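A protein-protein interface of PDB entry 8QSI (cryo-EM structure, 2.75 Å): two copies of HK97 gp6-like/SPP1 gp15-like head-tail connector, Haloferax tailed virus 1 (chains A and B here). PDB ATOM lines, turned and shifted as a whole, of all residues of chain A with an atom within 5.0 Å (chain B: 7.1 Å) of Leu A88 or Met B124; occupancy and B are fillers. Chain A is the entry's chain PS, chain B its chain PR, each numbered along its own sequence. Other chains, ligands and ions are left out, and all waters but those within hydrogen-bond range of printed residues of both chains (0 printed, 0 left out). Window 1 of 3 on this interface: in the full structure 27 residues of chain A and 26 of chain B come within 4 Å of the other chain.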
ATOM      1  N   HIS A  84       9.203  15.519 -29.356  1.00  0.00           N
ATOM      2  CA  HIS A  84       9.557  14.661 -28.235  1.00  0.00           C
ATOM      3  C   HIS A  84      10.988  14.927 -27.775  1.00  0.00           C
ATOM      4  O   HIS A  84      11.205  15.216 -26.604  1.00  0.00           O
ATOM      5  CB  HIS A  84       9.351  13.203 -28.623  1.00  0.00           C
ATOM      6  CG  HIS A  84       9.810  12.229 -27.598  1.00  0.00           C
ATOM      7  ND1 HIS A  84       9.147  11.966 -26.413  1.00  0.00           N
ATOM      8  CD2 HIS A  84      10.908  11.450 -27.601  1.00  0.00           C
ATOM      9  CE1 HIS A  84       9.824  11.048 -25.741  1.00  0.00           C
ATOM     10  NE2 HIS A  84      10.899  10.722 -26.447  1.00  0.00           N
ATOM     11  N   LYS A  85      11.940  14.934 -28.706  1.00  0.00           N
ATOM     12  CA  LYS A  85      13.334  15.176 -28.383  1.00  0.00           C
ATOM     13  C   LYS A  85      13.554  16.578 -27.829  1.00  0.00           C
ATOM     14  O   LYS A  85      14.202  16.703 -26.800  1.00  0.00           O
ATOM     15  CB  LYS A  85      14.220  14.836 -29.573  1.00  0.00           C
ATOM     16  CG  LYS A  85      14.200  13.348 -29.809  1.00  0.00           C
ATOM     17  CD  LYS A  85      15.080  12.862 -30.908  1.00  0.00           C
ATOM     18  CE  LYS A  85      15.080  11.352 -30.901  1.00  0.00           C
ATOM     19  NZ  LYS A  85      16.229  10.791 -31.649  1.00  0.00           N
ATOM     20  N   ILE A  86      12.961  17.617 -28.423  1.00  0.00           N
ATOM     21  CA  ILE A  86      13.101  18.965 -27.886  1.00  0.00           C
ATOM     22  C   ILE A  86      12.577  19.034 -26.452  1.00  0.00           C
ATOM     23  O   ILE A  86      13.217  19.619 -25.585  1.00  0.00           O
ATOM     24  CB  ILE A  86      12.442  20.023 -28.789  1.00  0.00           C
ATOM     25  CG1 ILE A  86      13.054  20.026 -30.188  1.00  0.00           C
ATOM     26  CG2 ILE A  86      12.564  21.402 -28.167  1.00  0.00           C
ATOM     27  CD1 ILE A  86      12.211  20.731 -31.222  1.00  0.00           C
ATOM     28  N   GLN A  87      11.452  18.388 -26.166  1.00  0.00           N
ATOM     29  CA  GLN A  87      10.914  18.380 -24.816  1.00  0.00           C
ATOM     30  C   GLN A  87      11.809  17.617 -23.833  1.00  0.00           C
ATOM     31  O   GLN A  87      11.909  18.010 -22.677  1.00  0.00           O
ATOM     32  CB  GLN A  87       9.497  17.830 -24.829  1.00  0.00           C
ATOM     33  CG  GLN A  87       8.773  18.072 -23.511  1.00  0.00           C
ATOM     34  CD  GLN A  87       8.595  19.542 -23.217  1.00  0.00           C
ATOM     35  OE1 GLN A  87       8.100  20.289 -24.054  1.00  0.00           O
ATOM     36  NE2 GLN A  87       9.002  19.994 -22.039  1.00  0.00           N
ATOM     37  N   LEU A  88      12.498  16.554 -24.266  1.00  0.00           N
ATOM     38  CA  LEU A  88      13.492  15.904 -23.419  1.00  0.00           C
ATOM     39  C   LEU A  88      14.746  16.762 -23.241  1.00  0.00           C
ATOM     40  O   LEU A  88      15.332  16.733 -22.164  1.00  0.00           O
ATOM     41  CB  LEU A  88      13.831  14.511 -23.952  1.00  0.00           C
ATOM     42  CG  LEU A  88      12.698  13.486 -23.929  1.00  0.00           C
ATOM     43  CD1 LEU A  88      13.241  12.115 -24.280  1.00  0.00           C
ATOM     44  CD2 LEU A  88      12.003  13.440 -22.572  1.00  0.00           C
ATOM     45  N   PHE A  89      15.133  17.572 -24.233  1.00  0.00           N
ATOM     46  CA  PHE A  89      16.233  18.517 -24.071  1.00  0.00           C
ATOM     47  C   PHE A  89      15.876  19.624 -23.069  1.00  0.00           C
ATOM     48  O   PHE A  89      16.766  20.169 -22.416  1.00  0.00           O
ATOM     49  CB  PHE A  89      16.662  19.108 -25.417  1.00  0.00           C
ATOM     50  CG  PHE A  89      17.153  18.169 -26.498  1.00  0.00           C
ATOM     51  CD1 PHE A  89      17.260  16.790 -26.312  1.00  0.00           C
ATOM     52  CD2 PHE A  89      17.543  18.687 -27.730  1.00  0.00           C
ATOM     53  CE1 PHE A  89      17.719  15.961 -27.336  1.00  0.00           C
ATOM     54  CE2 PHE A  89      18.001  17.861 -28.752  1.00  0.00           C
ATOM     55  CZ  PHE A  89      18.076  16.497 -28.561  1.00  0.00           C
ATOM     56  N   GLU A  90      14.584  19.934 -22.930  1.00  0.00           N
ATOM     57  CA  GLU A  90      14.058  20.880 -21.955  1.00  0.00           C
ATOM     58  C   GLU A  90      13.937  20.292 -20.541  1.00  0.00           C
ATOM     59  O   GLU A  90      13.374  20.936 -19.653  1.00  0.00           O
ATOM     60  CB  GLU A  90      12.706  21.384 -22.464  1.00  0.00           C
ATOM     61  CG  GLU A  90      12.844  22.350 -23.619  1.00  0.00           C
ATOM     62  CD  GLU A  90      12.986  23.779 -23.132  1.00  0.00           C
ATOM     63  OE1 GLU A  90      13.955  24.062 -22.386  1.00  0.00           O
ATOM     64  OE2 GLU A  90      12.116  24.612 -23.476  1.00  0.00           O
ATOM     65  N   GLY A  91      14.444  19.075 -20.313  1.00  0.00           N
ATOM     66  CA  GLY A  91      14.438  18.459 -18.996  1.00  0.00           C
ATOM     67  C   GLY A  91      13.332  17.425 -18.785  1.00  0.00           C
ATOM     68  O   GLY A  91      13.366  16.703 -17.791  1.00  0.00           O
ATOM     69  N   GLY A  92      12.369  17.345 -19.712  1.00  0.00           N
ATOM     70  CA  GLY A  92      11.266  16.394 -19.650  1.00  0.00           C
ATOM     71  C   GLY A  92       9.901  17.078 -19.697  1.00  0.00           C
ATOM     72  O   GLY A  92       9.800  18.295 -19.850  1.00  0.00           O
ATOM     73  N   ASP A 115      11.029   5.197 -23.561  1.00  0.00           N
ATOM     74  CA  ASP A 115      11.334   6.499 -24.138  1.00  0.00           C
ATOM     75  C   ASP A 115      10.097   7.239 -24.665  1.00  0.00           C
ATOM     76  O   ASP A 115       9.705   8.270 -24.124  1.00  0.00           O
ATOM     77  CB  ASP A 115      12.391   6.324 -25.224  1.00  0.00           C
ATOM     78  CG  ASP A 115      12.675   7.581 -26.027  1.00  0.00           C
ATOM     79  OD1 ASP A 115      12.530   8.684 -25.464  1.00  0.00           O
ATOM     80  OD2 ASP A 115      13.050   7.449 -27.213  1.00  0.00           O
ATOM     81  N   THR A 119       6.640  11.332 -22.930  1.00  0.00           N
ATOM     82  CA  THR A 119       6.204  12.684 -23.280  1.00  0.00           C
ATOM     83  C   THR A 119       4.939  12.603 -24.136  1.00  0.00           C
ATOM     84  O   THR A 119       4.791  11.654 -24.893  1.00  0.00           O
ATOM     85  CB  THR A 119       7.259  13.413 -24.128  1.00  0.00           C
ATOM     86  OG1 THR A 119       8.591  13.127 -23.710  1.00  0.00           O
ATOM     87  CG2 THR A 119       7.116  14.915 -24.113  1.00  0.00           C
ATOM     88  N   LEU B  32      22.372  18.362 -26.660  1.00  0.00           N
ATOM     89  CA  LEU B  32      21.330  17.475 -26.155  1.00  0.00           C
ATOM     90  C   LEU B  32      20.707  17.964 -24.842  1.00  0.00           C
ATOM     91  O   LEU B  32      19.809  17.319 -24.312  1.00  0.00           O
ATOM     92  CB  LEU B  32      21.865  16.047 -26.036  1.00  0.00           C
ATOM     93  CG  LEU B  32      22.395  15.446 -27.333  1.00  0.00           C
ATOM     94  CD1 LEU B  32      22.813  14.006 -27.101  1.00  0.00           C
ATOM     95  CD2 LEU B  32      21.370  15.515 -28.452  1.00  0.00           C
ATOM     96  N   SER B  33      21.136  19.115 -24.319  1.00  0.00           N
ATOM     97  CA  SER B  33      20.453  19.756 -23.209  1.00  0.00           C
ATOM     98  C   SER B  33      20.246  21.238 -23.501  1.00  0.00           C
ATOM     99  O   SER B  33      21.137  21.902 -24.028  1.00  0.00           O
ATOM    100  CB  SER B  33      21.208  19.555 -21.937  1.00  0.00           C
ATOM    101  OG  SER B  33      20.563  20.287 -20.909  1.00  0.00           O
ATOM    102  N   SER B  34      19.083  21.763 -23.102  1.00  0.00           N
ATOM    103  CA  SER B  34      18.794  23.189 -23.177  1.00  0.00           C
ATOM    104  C   SER B  34      19.785  24.006 -22.343  1.00  0.00           C
ATOM    105  O   SER B  34      20.120  25.128 -22.722  1.00  0.00           O
ATOM    106  CB  SER B  34      17.378  23.475 -22.766  1.00  0.00           C
ATOM    107  OG  SER B  34      17.123  22.887 -21.501  1.00  0.00           O
ATOM    108  N   TYR B  76      24.096   9.023 -32.934  1.00  0.00           N
ATOM    109  CA  TYR B  76      23.150   9.450 -31.917  1.00  0.00           C
ATOM    110  C   TYR B  76      23.098   8.512 -30.720  1.00  0.00           C
ATOM    111  O   TYR B  76      22.947   9.002 -29.612  1.00  0.00           O
ATOM    112  CB  TYR B  76      21.793   9.794 -32.517  1.00  0.00           C
ATOM    113  CG  TYR B  76      21.872  11.142 -33.181  1.00  0.00           C
ATOM    114  CD1 TYR B  76      22.018  12.281 -32.407  1.00  0.00           C
ATOM    115  CD2 TYR B  76      21.918  11.283 -34.564  1.00  0.00           C
ATOM    116  CE1 TYR B  76      22.181  13.534 -32.980  1.00  0.00           C
ATOM    117  CE2 TYR B  76      22.054  12.530 -35.154  1.00  0.00           C
ATOM    118  CZ  TYR B  76      22.182  13.660 -34.359  1.00  0.00           C
ATOM    119  OH  TYR B  76      22.338  14.892 -34.928  1.00  0.00           O
ATOM    120  N   PHE B  77      23.310   7.208 -30.899  1.00  0.00           N
ATOM    121  CA  PHE B  77      23.478   6.340 -29.743  1.00  0.00           C
ATOM    122  C   PHE B  77      24.640   6.791 -28.854  1.00  0.00           C
ATOM    123  O   PHE B  77      24.467   6.924 -27.644  1.00  0.00           O
ATOM    124  CB  PHE B  77      23.691   4.888 -30.146  1.00  0.00           C
ATOM    125  CG  PHE B  77      23.992   3.998 -28.960  1.00  0.00           C
ATOM    126  CD1 PHE B  77      23.007   3.705 -28.023  1.00  0.00           C
ATOM    127  CD2 PHE B  77      25.267   3.482 -28.745  1.00  0.00           C
ATOM    128  CE1 PHE B  77      23.268   2.895 -26.926  1.00  0.00           C
ATOM    129  CE2 PHE B  77      25.536   2.684 -27.635  1.00  0.00           C
ATOM    130  CZ  PHE B  77      24.535   2.388 -26.730  1.00  0.00           C
ATOM    131  N   TYR B  80      23.652  10.170 -27.082  1.00  0.00           N
ATOM    132  CA  TYR B  80      22.735   9.955 -25.968  1.00  0.00           C
ATOM    133  C   TYR B  80      23.426   9.253 -24.804  1.00  0.00           C
ATOM    134  O   TYR B  80      23.221   9.627 -23.658  1.00  0.00           O
ATOM    135  CB  TYR B  80      21.486   9.171 -26.381  1.00  0.00           C
ATOM    136  CG  TYR B  80      20.580   9.913 -27.327  1.00  0.00           C
ATOM    137  CD1 TYR B  80      20.187  11.221 -27.070  1.00  0.00           C
ATOM    138  CD2 TYR B  80      20.129   9.309 -28.494  1.00  0.00           C
ATOM    139  CE1 TYR B  80      19.398  11.928 -27.964  1.00  0.00           C
ATOM    140  CE2 TYR B  80      19.351  10.007 -29.399  1.00  0.00           C
ATOM    141  CZ  TYR B  80      18.979  11.316 -29.133  1.00  0.00           C
ATOM    142  OH  TYR B  80      18.194  11.991 -30.025  1.00  0.00           O
ATOM    143  N   ALA B  83      25.379  12.038 -23.132  1.00  0.00           N
ATOM    144  CA  ALA B  83      24.450  12.884 -22.398  1.00  0.00           C
ATOM    145  C   ALA B  83      23.960  12.199 -21.117  1.00  0.00           C
ATOM    146  O   ALA B  83      23.909  12.833 -20.068  1.00  0.00           O
ATOM    147  CB  ALA B  83      23.317  13.275 -23.315  1.00  0.00           C
ATOM    148  N   GLU B  93      18.969  12.764 -12.691  1.00  0.00           N
ATOM    149  CA  GLU B  93      17.885  13.498 -13.334  1.00  0.00           C
ATOM    150  C   GLU B  93      17.032  14.193 -12.268  1.00  0.00           C
ATOM    151  O   GLU B  93      16.511  13.529 -11.374  1.00  0.00           O
ATOM    152  CB  GLU B  93      17.078  12.508 -14.175  1.00  0.00           C
ATOM    153  CG  GLU B  93      15.926  13.107 -14.953  1.00  0.00           C
ATOM    154  CD  GLU B  93      15.700  12.356 -16.252  1.00  0.00           C
ATOM    155  OE1 GLU B  93      16.483  12.591 -17.204  1.00  0.00           O
ATOM    156  OE2 GLU B  93      14.807  11.479 -16.302  1.00  0.00           O
ATOM    157  N   LEU B 116      20.620   2.550 -17.714  1.00  0.00           N
ATOM    158  CA  LEU B 116      20.095   3.386 -18.786  1.00  0.00           C
ATOM    159  C   LEU B 116      18.637   3.795 -18.558  1.00  0.00           C
ATOM    160  O   LEU B 116      18.217   4.812 -19.076  1.00  0.00           O
ATOM    161  CB  LEU B 116      20.281   2.722 -20.151  1.00  0.00           C
ATOM    162  CG  LEU B 116      21.710   2.631 -20.677  1.00  0.00           C
ATOM    163  CD1 LEU B 116      21.732   1.877 -21.991  1.00  0.00           C
ATOM    164  CD2 LEU B 116      22.329   3.993 -20.898  1.00  0.00           C
ATOM    165  N   THR B 119      17.808   7.857 -16.576  1.00  0.00           N
ATOM    166  CA  THR B 119      17.628   9.224 -17.081  1.00  0.00           C
ATOM    167  C   THR B 119      17.025   9.228 -18.489  1.00  0.00           C
ATOM    168  O   THR B 119      17.109   8.232 -19.188  1.00  0.00           O
ATOM    169  CB  THR B 119      18.897  10.093 -17.021  1.00  0.00           C
ATOM    170  OG1 THR B 119      19.720   9.938 -18.170  1.00  0.00           O
ATOM    171  CG2 THR B 119      19.786   9.864 -15.819  1.00  0.00           C
ATOM    172  N   ARG B 120      16.476  10.363 -18.942  1.00  0.00           N
ATOM    173  CA  ARG B 120      15.831  10.509 -20.246  1.00  0.00           C
ATOM    174  C   ARG B 120      16.746  10.164 -21.425  1.00  0.00           C
ATOM    175  O   ARG B 120      16.307   9.518 -22.376  1.00  0.00           O
ATOM    176  CB  ARG B 120      15.207  11.901 -20.369  1.00  0.00           C
ATOM    177  CG  ARG B 120      16.194  13.054 -20.382  1.00  0.00           C
ATOM    178  CD  ARG B 120      15.564  14.334 -19.886  1.00  0.00           C
ATOM    179  NE  ARG B 120      16.476  15.461 -19.923  1.00  0.00           N
ATOM    180  CZ  ARG B 120      17.248  15.871 -18.924  1.00  0.00           C
ATOM    181  NH1 ARG B 120      18.002  16.943 -19.080  1.00  0.00           N
ATOM    182  NH2 ARG B 120      17.294  15.224 -17.776  1.00  0.00           N
ATOM    183  N   TYR B 121      18.022  10.542 -21.347  1.00  0.00           N
ATOM    184  CA  TYR B 121      18.991  10.221 -22.379  1.00  0.00           C
ATOM    185  C   TYR B 121      19.288   8.727 -22.447  1.00  0.00           C
ATOM    186  O   TYR B 121      19.471   8.187 -23.532  1.00  0.00           O
ATOM    187  CB  TYR B 121      20.265  11.018 -22.143  1.00  0.00           C
ATOM    188  CG  TYR B 121      20.009  12.492 -22.037  1.00  0.00           C
ATOM    189  CD1 TYR B 121      19.562  13.188 -23.146  1.00  0.00           C
ATOM    190  CD2 TYR B 121      20.168  13.181 -20.842  1.00  0.00           C
ATOM    191  CE1 TYR B 121      19.278  14.539 -23.075  1.00  0.00           C
ATOM    192  CE2 TYR B 121      19.877  14.538 -20.753  1.00  0.00           C
ATOM    193  CZ  TYR B 121      19.434  15.215 -21.879  1.00  0.00           C
ATOM    194  OH  TYR B 121      19.156  16.547 -21.843  1.00  0.00           O
ATOM    195  N   GLY B 122      19.317   8.051 -21.299  1.00  0.00           N
ATOM    196  CA  GLY B 122      19.517   6.614 -21.256  1.00  0.00           C
ATOM    197  C   GLY B 122      18.301   5.856 -21.786  1.00  0.00           C
ATOM    198  O   GLY B 122      18.462   4.884 -22.513  1.00  0.00           O
ATOM    199  N   ARG B 123      17.091   6.343 -21.489  1.00  0.00           N
ATOM    200  CA  ARG B 123      15.864   5.799 -22.051  1.00  0.00           C
ATOM    201  C   ARG B 123      15.854   5.936 -23.571  1.00  0.00           C
ATOM    202  O   ARG B 123      15.521   4.972 -24.244  1.00  0.00           O
ATOM    203  CB  ARG B 123      14.637   6.408 -21.377  1.00  0.00           C
ATOM    204  CG  ARG B 123      14.507   5.984 -19.926  1.00  0.00           C
ATOM    205  CD  ARG B 123      13.236   6.474 -19.281  1.00  0.00           C
ATOM    206  NE  ARG B 123      13.124   7.910 -19.068  1.00  0.00           N
ATOM    207  CZ  ARG B 123      13.464   8.575 -17.972  1.00  0.00           C
ATOM    208  NH1 ARG B 123      13.227   9.873 -17.908  1.00  0.00           N
ATOM    209  NH2 ARG B 123      14.050   7.983 -16.948  1.00  0.00           N
ATOM    210  N   MET B 124      16.286   7.077 -24.118  1.00  0.00           N
ATOM    211  CA  MET B 124      16.490   7.209 -25.556  1.00  0.00           C
ATOM    212  C   MET B 124      17.527   6.216 -26.082  1.00  0.00           C
ATOM    213  O   MET B 124      17.258   5.530 -27.057  1.00  0.00           O
ATOM    214  CB  MET B 124      16.874   8.632 -25.960  1.00  0.00           C
ATOM    215  CG  MET B 124      15.668   9.540 -25.968  1.00  0.00           C
ATOM    216  SD  MET B 124      15.953  11.158 -26.709  1.00  0.00           S
ATOM    217  CE  MET B 124      16.887  11.981 -25.419  1.00  0.00           C
ATOM    218  N   ALA B 125      18.691   6.098 -25.435  1.00  0.00           N
ATOM    219  CA  ALA B 125      19.760   5.216 -25.883  1.00  0.00           C
ATOM    220  C   ALA B 125      19.311   3.751 -25.966  1.00  0.00           C
ATOM    221  O   ALA B 125      19.660   3.062 -26.914  1.00  0.00           O
ATOM    222  CB  ALA B 125      20.945   5.384 -24.963  1.00  0.00           C
ATOM    223  N   LEU B 126      18.496   3.267 -25.021  1.00  0.00           N
ATOM    224  CA  LEU B 126      18.026   1.886 -25.004  1.00  0.00           C
ATOM    225  C   LEU B 126      17.315   1.471 -26.290  1.00  0.00           C
ATOM    226  O   LEU B 126      17.488   0.340 -26.722  1.00  0.00           O
ATOM    227  CB  LEU B 126      17.102   1.667 -23.811  1.00  0.00           C
ATOM    228  CG  LEU B 126      17.816   1.406 -22.492  1.00  0.00           C
ATOM    229  CD1 LEU B 126      16.839   1.544 -21.333  1.00  0.00           C
ATOM    230  CD2 LEU B 126      18.471   0.026 -22.489  1.00  0.00           C
ATOM    231  N   GLU B 127      16.553   2.363 -26.929  1.00  0.00           N
ATOM    232  CA  GLU B 127      15.852   2.039 -28.161  1.00  0.00           C
ATOM    233  C   GLU B 127      16.815   1.686 -29.302  1.00  0.00           C
ATOM    234  O   GLU B 127      16.445   0.950 -30.211  1.00  0.00           O
ATOM    235  CB  GLU B 127      14.886   3.165 -28.526  1.00  0.00           C
ATOM    236  CG  GLU B 127      13.658   3.237 -27.620  1.00  0.00           C
ATOM    237  CD  GLU B 127      12.502   2.265 -27.868  1.00  0.00           C
ATOM    238  OE1 GLU B 127      12.514   1.525 -28.885  1.00  0.00           O
ATOM    239  OE2 GLU B 127      11.568   2.215 -27.032  1.00  0.00           O
ATOM    240  N   TYR B 128      18.061   2.167 -29.245  1.00  0.00           N
ATOM    241  CA  TYR B 128      19.066   1.910 -30.272  1.00  0.00           C
ATOM    242  C   TYR B 128      19.694   0.519 -30.141  1.00  0.00           C
ATOM    243  O   TYR B 128      20.322   0.045 -31.083  1.00  0.00           O
ATOM    244  CB  TYR B 128      20.146   3.000 -30.244  1.00  0.00           C
ATOM    245  CG  TYR B 128      19.679   4.366 -30.691  1.00  0.00           C
ATOM    246  CD1 TYR B 128      18.743   5.081 -29.944  1.00  0.00           C
ATOM    247  CD2 TYR B 128      20.173   4.955 -31.857  1.00  0.00           C
ATOM    248  CE1 TYR B 128      18.268   6.318 -30.376  1.00  0.00           C
ATOM    249  CE2 TYR B 128      19.694   6.182 -32.304  1.00  0.00           C
ATOM    250  CZ  TYR B 128      18.731   6.858 -31.564  1.00  0.00           C
ATOM    251  OH  TYR B 128      18.207   8.037 -32.010  1.00  0.00           O
ATOM    252  N   VAL B 129      19.543  -0.132 -28.980  1.00  0.00           N
ATOM    253  CA  VAL B 129      20.225  -1.377 -28.642  1.00  0.00           C
ATOM    254  C   VAL B 129      19.222  -2.443 -28.204  1.00  0.00           C
ATOM    255  O   VAL B 129      19.422  -3.127 -27.201  1.00  0.00           O
ATOM    256  CB  VAL B 129      21.345  -1.152 -27.603  1.00  0.00           C
ATOM    257  CG1 VAL B 129      22.487  -0.371 -28.218  1.00  0.00           C
ATOM    258  CG2 VAL B 129      20.873  -0.436 -26.344  1.00  0.00           C
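NZ of Lys A85 is in hydrogen-bond range of OH of Tyr B80, at 2.8 Å. The side-chain carboxylate (OE1) of Glu A90 lies within hydrogen-bond range of the side-chain hydroxyl (OG) of Ser B34 (3.5 Å). The backbone carbonyl oxygen (O) of Leu A88 sits at hydrogen-bond distance from the guanidinium group (NE) of Arg B120 (2.8 Å). The backbone carbonyl oxygen (O) of Phe A89 lies within hydrogen-bond range of the side-chain hydroxyl (OG) of Ser B34, at 2.9 Å. The side-chain amino group (NZ) of Lys A85 sits at hydrogen-bond distance from the side-chain hydroxyl (OH) of Tyr B128 (3.4 Å).
The side-chain carboxylate (OE1) of Glu B93 is in salt-bridge range of the guanidinium group (NH2) of Arg B120, 2.8 Å away. NE2 of His A84 sits at hydrogen-bond distance from OD1 of Asp A115, at 2.8 Å. The guanidinium group (NH1) of Arg B123 is in salt-bridge range of the side-chain carboxylate (OE2) of Glu B93, 2.8 Å away. OH of Tyr B121 is in hydrogen-bond range of NH1 of Arg B120 (3.0 Å). The backbone carbonyl oxygen of Leu B32 is in hydrogen-bond range of the side-chain hydroxyl of Tyr B121. O of Leu B116 lies within hydrogen-bond range of N of Arg B123.
Among the printed residues, pairs that only touch across the chains: Phe A89 with Leu B32, Asp A115 with Met B124, Asp A115 with Arg B123, Gly A91 with Arg B120, Leu A88 with Met B124, Phe A89 with Ser B33 and Leu A88 with Tyr B121.
Printed residues of chain B within 4 Å of Lys A85: Tyr B80 and Tyr B128. Printed residues of chain B within 4 Å of Glu A90: Ser B34 (3.5 Å). Glu B93 touches none of the printed residues of chain A. Printed residues of chain A within 4 Å of Tyr B121: Leu A88. Printed residues of chain A within 4 Å of Arg B123: Asp A115 (3.5 Å). Of chain A, only Leu A88 (3.8 Å) and Asp A115 (3.3 Å) come within 4 Å of Met B124. Val B129 touches none of the printed residues of chain A. The nearest residue of chain B that does not touch Leu A88 is Leu B32 (5.0 Å). The nearest printed residue of chain A that does not touch Tyr B121 is Phe A89 (4.2 Å).
Of the 20 printed residues of chain B, 9 touch a printed residue of chain A. Printed residues of chain B that touch a printed residue of chain A: Leu B32, Ser B33, Ser B34, Tyr B80, Arg B120, Tyr B121, Arg B123, Met B124 and Tyr B128. Hydrophobic or aromatic side chains of chain B that line the printed part of chain A: Leu B32, Tyr B80, Tyr B121, Met B124 and Tyr B128. Of the 11 printed residues of chain A, 6 touch a printed residue of chain B. Hydrophobic or aromatic side chains of chain A within 4 Å of the printed part of chain B: Leu A88 and Phe A89.
Position printed for both chains: 119. Of the 12 pairs that touch across the chains among the printed residues, none has its exchanged pair printed and touching as well.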
